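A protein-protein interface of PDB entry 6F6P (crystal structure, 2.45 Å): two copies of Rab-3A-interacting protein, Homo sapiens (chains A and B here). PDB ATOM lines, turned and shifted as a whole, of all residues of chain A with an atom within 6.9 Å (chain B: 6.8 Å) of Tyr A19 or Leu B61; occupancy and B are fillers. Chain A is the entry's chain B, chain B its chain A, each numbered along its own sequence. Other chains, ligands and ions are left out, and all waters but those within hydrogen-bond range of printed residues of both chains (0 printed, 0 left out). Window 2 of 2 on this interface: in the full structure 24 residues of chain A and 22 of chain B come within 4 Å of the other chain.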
ATOM      1  N   VAL A  14       9.701   6.160  10.905  1.00  0.00           N
ATOM      2  CA  VAL A  14       8.241   6.180  10.864  1.00  0.00           C
ATOM      3  C   VAL A  14       7.705   7.355  11.672  1.00  0.00           C
ATOM      4  O   VAL A  14       6.964   8.206  11.157  1.00  0.00           O
ATOM      5  CB  VAL A  14       7.668   4.844  11.370  1.00  0.00           C
ATOM      6  CG1 VAL A  14       6.153   4.920  11.469  1.00  0.00           C
ATOM      7  CG2 VAL A  14       8.087   3.704  10.453  1.00  0.00           C
ATOM      8  N   ARG A  15       8.081   7.424  12.955  1.00  0.00           N
ATOM      9  CA  ARG A  15       7.563   8.493  13.806  1.00  0.00           C
ATOM     10  C   ARG A  15       8.002   9.864  13.306  1.00  0.00           C
ATOM     11  O   ARG A  15       7.231  10.830  13.361  1.00  0.00           O
ATOM     12  CB  ARG A  15       8.005   8.273  15.252  1.00  0.00           C
ATOM     13  CG  ARG A  15       7.174   7.232  15.976  1.00  0.00           C
ATOM     14  CD  ARG A  15       8.045   6.177  16.619  1.00  0.00           C
ATOM     15  NE  ARG A  15       7.249   5.072  17.149  1.00  0.00           N
ATOM     16  CZ  ARG A  15       6.812   4.051  16.421  1.00  0.00           C
ATOM     17  NH1 ARG A  15       6.097   3.088  16.987  1.00  0.00           N
ATOM     18  NH2 ARG A  15       7.094   3.988  15.126  1.00  0.00           N
ATOM     19  N   GLU A  16       9.235   9.966  12.808  1.00  0.00           N
ATOM     20  CA  GLU A  16       9.694  11.217  12.216  1.00  0.00           C
ATOM     21  C   GLU A  16       8.884  11.573  10.977  1.00  0.00           C
ATOM     22  O   GLU A  16       8.570  12.746  10.749  1.00  0.00           O
ATOM     23  CB  GLU A  16      11.181  11.130  11.872  1.00  0.00           C
ATOM     24  CG  GLU A  16      12.109  11.572  12.993  1.00  0.00           C
ATOM     25  CD  GLU A  16      13.565  11.592  12.568  1.00  0.00           C
ATOM     26  OE1 GLU A  16      13.875  11.058  11.482  1.00  0.00           O
ATOM     27  OE2 GLU A  16      14.397  12.142  13.318  1.00  0.00           O
ATOM     28  N   LYS A  17       8.548  10.576  10.154  1.00  0.00           N
ATOM     29  CA  LYS A  17       7.760  10.845   8.955  1.00  0.00           C
ATOM     30  C   LYS A  17       6.378  11.388   9.303  1.00  0.00           C
ATOM     31  O   LYS A  17       5.940  12.401   8.742  1.00  0.00           O
ATOM     32  CB  LYS A  17       7.646   9.575   8.111  1.00  0.00           C
ATOM     33  CG  LYS A  17       8.402   9.635   6.794  1.00  0.00           C
ATOM     34  CD  LYS A  17       9.870   9.961   7.012  1.00  0.00           C
ATOM     35  CE  LYS A  17      10.614  10.069   5.690  1.00  0.00           C
ATOM     36  NZ  LYS A  17      12.046  10.428   5.885  1.00  0.00           N
ATOM     37  N   GLY A  18       5.678  10.740  10.239  1.00  0.00           N
ATOM     38  CA  GLY A  18       4.362  11.235  10.615  1.00  0.00           C
ATOM     39  C   GLY A  18       4.409  12.583  11.315  1.00  0.00           C
ATOM     40  O   GLY A  18       3.590  13.472  11.038  1.00  0.00           O
ATOM     41  N   TYR A  19       5.397  12.772  12.192  1.00  0.00           N
ATOM     42  CA  TYR A  19       5.515  14.021  12.937  1.00  0.00           C
ATOM     43  C   TYR A  19       5.824  15.182  12.001  1.00  0.00           C
ATOM     44  O   TYR A  19       5.203  16.247  12.088  1.00  0.00           O
ATOM     45  CB  TYR A  19       6.593  13.883  14.013  1.00  0.00           C
ATOM     46  CG  TYR A  19       6.786  15.119  14.863  1.00  0.00           C
ATOM     47  CD1 TYR A  19       5.951  15.376  15.941  1.00  0.00           C
ATOM     48  CD2 TYR A  19       7.804  16.023  14.591  1.00  0.00           C
ATOM     49  CE1 TYR A  19       6.121  16.500  16.725  1.00  0.00           C
ATOM     50  CE2 TYR A  19       7.981  17.153  15.368  1.00  0.00           C
ATOM     51  CZ  TYR A  19       7.137  17.385  16.434  1.00  0.00           C
ATOM     52  OH  TYR A  19       7.308  18.507  17.213  1.00  0.00           O
ATOM     53  N   GLU A  20       6.787  14.990  11.099  1.00  0.00           N
ATOM     54  CA  GLU A  20       7.122  16.033  10.138  1.00  0.00           C
ATOM     55  C   GLU A  20       5.976  16.284   9.169  1.00  0.00           C
ATOM     56  O   GLU A  20       5.798  17.417   8.709  1.00  0.00           O
ATOM     57  CB  GLU A  20       8.398  15.667   9.379  1.00  0.00           C
ATOM     58  CG  GLU A  20       9.660  15.759  10.222  1.00  0.00           C
ATOM     59  CD  GLU A  20       9.918  17.165  10.733  1.00  0.00           C
ATOM     60  OE1 GLU A  20       9.590  18.132  10.014  1.00  0.00           O
ATOM     61  OE2 GLU A  20      10.447  17.303  11.856  1.00  0.00           O
ATOM     62  N   ARG A  21       5.212  15.246   8.823  1.00  0.00           N
ATOM     63  CA  ARG A  21       4.049  15.448   7.964  1.00  0.00           C
ATOM     64  C   ARG A  21       3.036  16.379   8.623  1.00  0.00           C
ATOM     65  O   ARG A  21       2.648  17.408   8.048  1.00  0.00           O
ATOM     66  CB  ARG A  21       3.410  14.100   7.629  1.00  0.00           C
ATOM     67  CG  ARG A  21       2.234  14.185   6.669  1.00  0.00           C
ATOM     68  CD  ARG A  21       1.638  12.811   6.377  1.00  0.00           C
ATOM     69  NE  ARG A  21       2.621  11.878   5.831  1.00  0.00           N
ATOM     70  CZ  ARG A  21       3.143  10.859   6.509  1.00  0.00           C
ATOM     71  NH1 ARG A  21       2.775  10.635   7.762  1.00  0.00           N
ATOM     72  NH2 ARG A  21       4.031  10.062   5.930  1.00  0.00           N
ATOM     73  N   LEU A  22       2.606  16.044   9.846  1.00  0.00           N
ATOM     74  CA  LEU A  22       1.629  16.888  10.532  1.00  0.00           C
ATOM     75  C   LEU A  22       2.182  18.286  10.796  1.00  0.00           C
ATOM     76  O   LEU A  22       1.463  19.286  10.658  1.00  0.00           O
ATOM     77  CB  LEU A  22       1.196  16.228  11.841  1.00  0.00           C
ATOM     78  CG  LEU A  22       0.197  16.998  12.708  1.00  0.00           C
ATOM     79  CD1 LEU A  22      -1.025  17.401  11.898  1.00  0.00           C
ATOM     80  CD2 LEU A  22      -0.208  16.170  13.919  1.00  0.00           C
ATOM     81  N   LYS A  23       3.465  18.375  11.158  1.00  0.00           N
ATOM     82  CA  LYS A  23       4.086  19.676  11.393  1.00  0.00           C
ATOM     83  C   LYS A  23       4.083  20.524  10.127  1.00  0.00           C
ATOM     84  O   LYS A  23       3.800  21.728  10.174  1.00  0.00           O
ATOM     85  CB  LYS A  23       5.507  19.486  11.927  1.00  0.00           C
ATOM     86  CG  LYS A  23       6.276  20.777  12.144  1.00  0.00           C
ATOM     87  CD  LYS A  23       7.589  20.512  12.862  1.00  0.00           C
ATOM     88  CE  LYS A  23       8.669  21.491  12.436  1.00  0.00           C
ATOM     89  NZ  LYS A  23       9.981  21.173  13.064  1.00  0.00           N
ATOM     90  N   GLU A  24       4.387  19.908   8.982  1.00  0.00           N
ATOM     91  CA  GLU A  24       4.369  20.633   7.716  1.00  0.00           C
ATOM     92  C   GLU A  24       2.963  21.111   7.382  1.00  0.00           C
ATOM     93  O   GLU A  24       2.782  22.236   6.897  1.00  0.00           O
ATOM     94  CB  GLU A  24       4.911  19.742   6.599  1.00  0.00           C
ATOM     95  CG  GLU A  24       4.971  20.408   5.236  1.00  0.00           C
ATOM     96  CD  GLU A  24       5.691  19.560   4.205  1.00  0.00           C
ATOM     97  OE1 GLU A  24       6.152  18.454   4.558  1.00  0.00           O
ATOM     98  OE2 GLU A  24       5.797  20.000   3.041  1.00  0.00           O
ATOM     99  N   GLU A  25       1.953  20.281   7.658  1.00  0.00           N
ATOM    100  CA  GLU A  25       0.578  20.710   7.428  1.00  0.00           C
ATOM    101  C   GLU A  25       0.242  21.925   8.289  1.00  0.00           C
ATOM    102  O   GLU A  25      -0.377  22.892   7.813  1.00  0.00           O
ATOM    103  CB  GLU A  25      -0.379  19.552   7.719  1.00  0.00           C
ATOM    104  CG  GLU A  25      -1.841  19.856   7.471  1.00  0.00           C
ATOM    105  CD  GLU A  25      -2.118  20.195   6.020  1.00  0.00           C
ATOM    106  OE1 GLU A  25      -1.463  19.603   5.136  1.00  0.00           O
ATOM    107  OE2 GLU A  25      -2.994  21.046   5.762  1.00  0.00           O
ATOM    108  N   LEU B  54      -1.021  18.247  16.877  1.00  0.00           N
ATOM    109  CA  LEU B  54       0.427  18.131  17.011  1.00  0.00           C
ATOM    110  C   LEU B  54       0.844  18.002  18.470  1.00  0.00           C
ATOM    111  O   LEU B  54       1.814  17.298  18.779  1.00  0.00           O
ATOM    112  CB  LEU B  54       1.110  19.340  16.368  1.00  0.00           C
ATOM    113  CG  LEU B  54       2.638  19.321  16.315  1.00  0.00           C
ATOM    114  CD1 LEU B  54       3.135  18.120  15.526  1.00  0.00           C
ATOM    115  CD2 LEU B  54       3.175  20.616  15.723  1.00  0.00           C
ATOM    116  N   GLU B  56      -0.973  16.486  20.842  1.00  0.00           N
ATOM    117  CA  GLU B  56      -1.278  15.106  21.210  1.00  0.00           C
ATOM    118  C   GLU B  56      -0.229  14.145  20.662  1.00  0.00           C
ATOM    119  O   GLU B  56       0.250  13.254  21.376  1.00  0.00           O
ATOM    120  CB  GLU B  56      -2.671  14.731  20.704  1.00  0.00           C
ATOM    121  CG  GLU B  56      -3.791  15.582  21.279  1.00  0.00           C
ATOM    122  CD  GLU B  56      -5.145  15.243  20.687  1.00  0.00           C
ATOM    123  OE1 GLU B  56      -5.228  14.273  19.904  1.00  0.00           O
ATOM    124  OE2 GLU B  56      -6.128  15.947  21.002  1.00  0.00           O
ATOM    125  N   LEU B  57       0.143  14.313  19.388  1.00  0.00           N
ATOM    126  CA  LEU B  57       1.168  13.453  18.802  1.00  0.00           C
ATOM    127  C   LEU B  57       2.496  13.588  19.538  1.00  0.00           C
ATOM    128  O   LEU B  57       3.189  12.588  19.774  1.00  0.00           O
ATOM    129  CB  LEU B  57       1.342  13.781  17.320  1.00  0.00           C
ATOM    130  CG  LEU B  57       2.359  12.934  16.552  1.00  0.00           C
ATOM    131  CD1 LEU B  57       2.012  11.456  16.652  1.00  0.00           C
ATOM    132  CD2 LEU B  57       2.439  13.373  15.099  1.00  0.00           C
ATOM    133  N   THR B  58       2.863  14.814  19.922  1.00  0.00           N
ATOM    134  CA  THR B  58       4.106  15.022  20.659  1.00  0.00           C
ATOM    135  C   THR B  58       4.077  14.294  22.000  1.00  0.00           C
ATOM    136  O   THR B  58       5.037  13.604  22.371  1.00  0.00           O
ATOM    137  CB  THR B  58       4.348  16.519  20.860  1.00  0.00           C
ATOM    138  OG1 THR B  58       4.536  17.150  19.587  1.00  0.00           O
ATOM    139  CG2 THR B  58       5.579  16.755  21.719  1.00  0.00           C
ATOM    140  N   ALA B  59       2.971  14.433  22.737  1.00  0.00           N
ATOM    141  CA  ALA B  59       2.835  13.730  24.008  1.00  0.00           C
ATOM    142  C   ALA B  59       2.952  12.222  23.818  1.00  0.00           C
ATOM    143  O   ALA B  59       3.640  11.541  24.590  1.00  0.00           O
ATOM    144  CB  ALA B  59       1.504  14.088  24.667  1.00  0.00           C
ATOM    145  N   SER B  60       2.285  11.684  22.792  1.00  0.00           N
ATOM    146  CA  SER B  60       2.381  10.254  22.516  1.00  0.00           C
ATOM    147  C   SER B  60       3.820   9.837  22.236  1.00  0.00           C
ATOM    148  O   SER B  60       4.266   8.776  22.694  1.00  0.00           O
ATOM    149  CB  SER B  60       1.478   9.886  21.338  1.00  0.00           C
ATOM    150  OG  SER B  60       0.112  10.083  21.662  1.00  0.00           O
ATOM    151  N   LEU B  61       4.563  10.656  21.487  1.00  0.00           N
ATOM    152  CA  LEU B  61       5.948  10.310  21.182  1.00  0.00           C
ATOM    153  C   LEU B  61       6.815  10.312  22.437  1.00  0.00           C
ATOM    154  O   LEU B  61       7.671   9.434  22.609  1.00  0.00           O
ATOM    155  CB  LEU B  61       6.514  11.278  20.143  1.00  0.00           C
ATOM    156  CG  LEU B  61       5.924  11.198  18.734  1.00  0.00           C
ATOM    157  CD1 LEU B  61       6.676  12.119  17.782  1.00  0.00           C
ATOM    158  CD2 LEU B  61       5.939   9.766  18.228  1.00  0.00           C
ATOM    159  N   PHE B  62       6.597  11.277  23.334  1.00  0.00           N
ATOM    160  CA  PHE B  62       7.369  11.308  24.575  1.00  0.00           C
ATOM    161  C   PHE B  62       7.051  10.103  25.453  1.00  0.00           C
ATOM    162  O   PHE B  62       7.960   9.450  25.986  1.00  0.00           O
ATOM    163  CB  PHE B  62       7.101  12.613  25.324  1.00  0.00           C
ATOM    164  CG  PHE B  62       7.898  13.777  24.811  1.00  0.00           C
ATOM    165  CD1 PHE B  62       9.236  13.628  24.489  1.00  0.00           C
ATOM    166  CD2 PHE B  62       7.308  15.020  24.647  1.00  0.00           C
ATOM    167  CE1 PHE B  62       9.973  14.696  24.015  1.00  0.00           C
ATOM    168  CE2 PHE B  62       8.040  16.093  24.174  1.00  0.00           C
ATOM    169  CZ  PHE B  62       9.373  15.930  23.857  1.00  0.00           C
ATOM    170  N   GLU B  63       5.761   9.787  25.603  1.00  0.00           N
ATOM    171  CA  GLU B  63       5.369   8.615  26.380  1.00  0.00           C
ATOM    172  C   GLU B  63       5.975   7.343  25.801  1.00  0.00           C
ATOM    173  O   GLU B  63       6.455   6.479  26.546  1.00  0.00           O
ATOM    174  CB  GLU B  63       3.846   8.509  26.439  1.00  0.00           C
ATOM    175  CG  GLU B  63       3.178   9.630  27.219  1.00  0.00           C
ATOM    176  CD  GLU B  63       1.680   9.441  27.346  1.00  0.00           C
ATOM    177  OE1 GLU B  63       1.227   8.278  27.392  1.00  0.00           O
ATOM    178  OE2 GLU B  63       0.954  10.456  27.400  1.00  0.00           O
ATOM    179  N   GLU B  64       5.960   7.207  24.472  1.00  0.00           N
ATOM    180  CA  GLU B  64       6.564   6.036  23.845  1.00  0.00           C
ATOM    181  C   GLU B  64       8.060   5.976  24.122  1.00  0.00           C
ATOM    182  O   GLU B  64       8.614   4.895  24.367  1.00  0.00           O
ATOM    183  CB  GLU B  64       6.294   6.047  22.341  1.00  0.00           C
ATOM    184  CG  GLU B  64       6.743   4.786  21.622  1.00  0.00           C
ATOM    185  CD  GLU B  64       6.285   4.745  20.179  1.00  0.00           C
ATOM    186  OE1 GLU B  64       5.818   5.786  19.670  1.00  0.00           O
ATOM    187  OE2 GLU B  64       6.389   3.670  19.551  1.00  0.00           O
ATOM    188  N   ALA B  65       8.735   7.130  24.096  1.00  0.00           N
ATOM    189  CA  ALA B  65      10.166   7.157  24.374  1.00  0.00           C
ATOM    190  C   ALA B  65      10.460   6.692  25.802  1.00  0.00           C
ATOM    191  O   ALA B  65      11.329   5.846  26.024  1.00  0.00           O
ATOM    192  CB  ALA B  65      10.723   8.560  24.136  1.00  0.00           C
ATOM    193  N   HIS B  66       9.726   7.247  26.773  1.00  0.00           N
ATOM    194  CA  HIS B  66       9.923   6.845  28.164  1.00  0.00           C
ATOM    195  C   HIS B  66       9.608   5.368  28.364  1.00  0.00           C
ATOM    196  O   HIS B  66      10.272   4.685  29.155  1.00  0.00           O
ATOM    197  CB  HIS B  66       9.058   7.710  29.083  1.00  0.00           C
ATOM    198  CG  HIS B  66       9.178   7.359  30.533  1.00  0.00           C
ATOM    199  ND1 HIS B  66      10.344   7.530  31.247  1.00  0.00           N
ATOM    200  CD2 HIS B  66       8.276   6.847  31.405  1.00  0.00           C
ATOM    201  CE1 HIS B  66      10.157   7.138  32.495  1.00  0.00           C
ATOM    202  NE2 HIS B  66       8.909   6.720  32.616  1.00  0.00           N
ATOM    203  N   MET B  68       9.938   2.916  26.067  1.00  0.00           N
ATOM    204  CA  MET B  68      11.044   2.138  25.518  1.00  0.00           C
ATOM    205  C   MET B  68      12.245   2.166  26.454  1.00  0.00           C
ATOM    206  O   MET B  68      12.904   1.138  26.666  1.00  0.00           O
ATOM    207  CB  MET B  68      11.432   2.661  24.134  1.00  0.00           C
ATOM    208  CG  MET B  68      10.390   2.412  23.055  1.00  0.00           C
ATOM    209  SD  MET B  68      10.864   3.091  21.451  1.00  0.00           S
ATOM    210  CE  MET B  68      11.274   4.776  21.892  1.00  0.00           C
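OE2 of Glu B64 lies within salt-bridge range of NH1 of Arg A15 (2.6 Å).
Printed residues of chain B that touch a printed residue of chain A: Leu B54, Leu B57, Thr B58, Leu B61 and Glu B64.
Hydrophobic or aromatic side chains of chain B within 4 Å of the printed part of chain A: Leu B54, Leu B57 and Leu B61.
Hydrophobic or aromatic side chains of chain A that line the printed part of chain B: Tyr A19 and Leu A22.
Among the printed residues, Asp or Glu carboxylates within 4 Å of a Lys or Arg side-chain nitrogen of the other chain: Arg A15 with Glu B64 (2.6 Å).
CD2 of Leu B61 touches CG of Arg A15 (3.6 Å).
Leu B54 touches Tyr A19 (CD1 to CE1, 3.6 Å).
CA of Tyr A19 touches CD2 of Leu B57 (3.8 Å).
CE1 of Tyr A19 touches OG1 of Thr B58, at 3.3 Å.
Leu B61 touches Tyr A19.
Leu A22 touches Leu B54.
OG1 of Thr B58 is in hydrogen-bond range of O of Leu B54 (2.8 Å).
Printed residues of chain B within 4 Å of Tyr A19: Leu B54, Leu B57, Thr B58 and Leu B61.
Of chain A, only Arg A15 (3.6 Å) and Tyr A19 (3.8 Å) come within 4 Å of Leu B61.
Of the printed residues of chain B, Arg A15 touches Leu B61 (3.6 Å) and Glu B64 (2.6 Å).
Of the printed residues of chain A, Thr B58 touches Tyr A19.
The nearest printed residue of chain B that does not touch Tyr A19 is Ala B59 (7.1 Å).
No position is printed for both chains.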
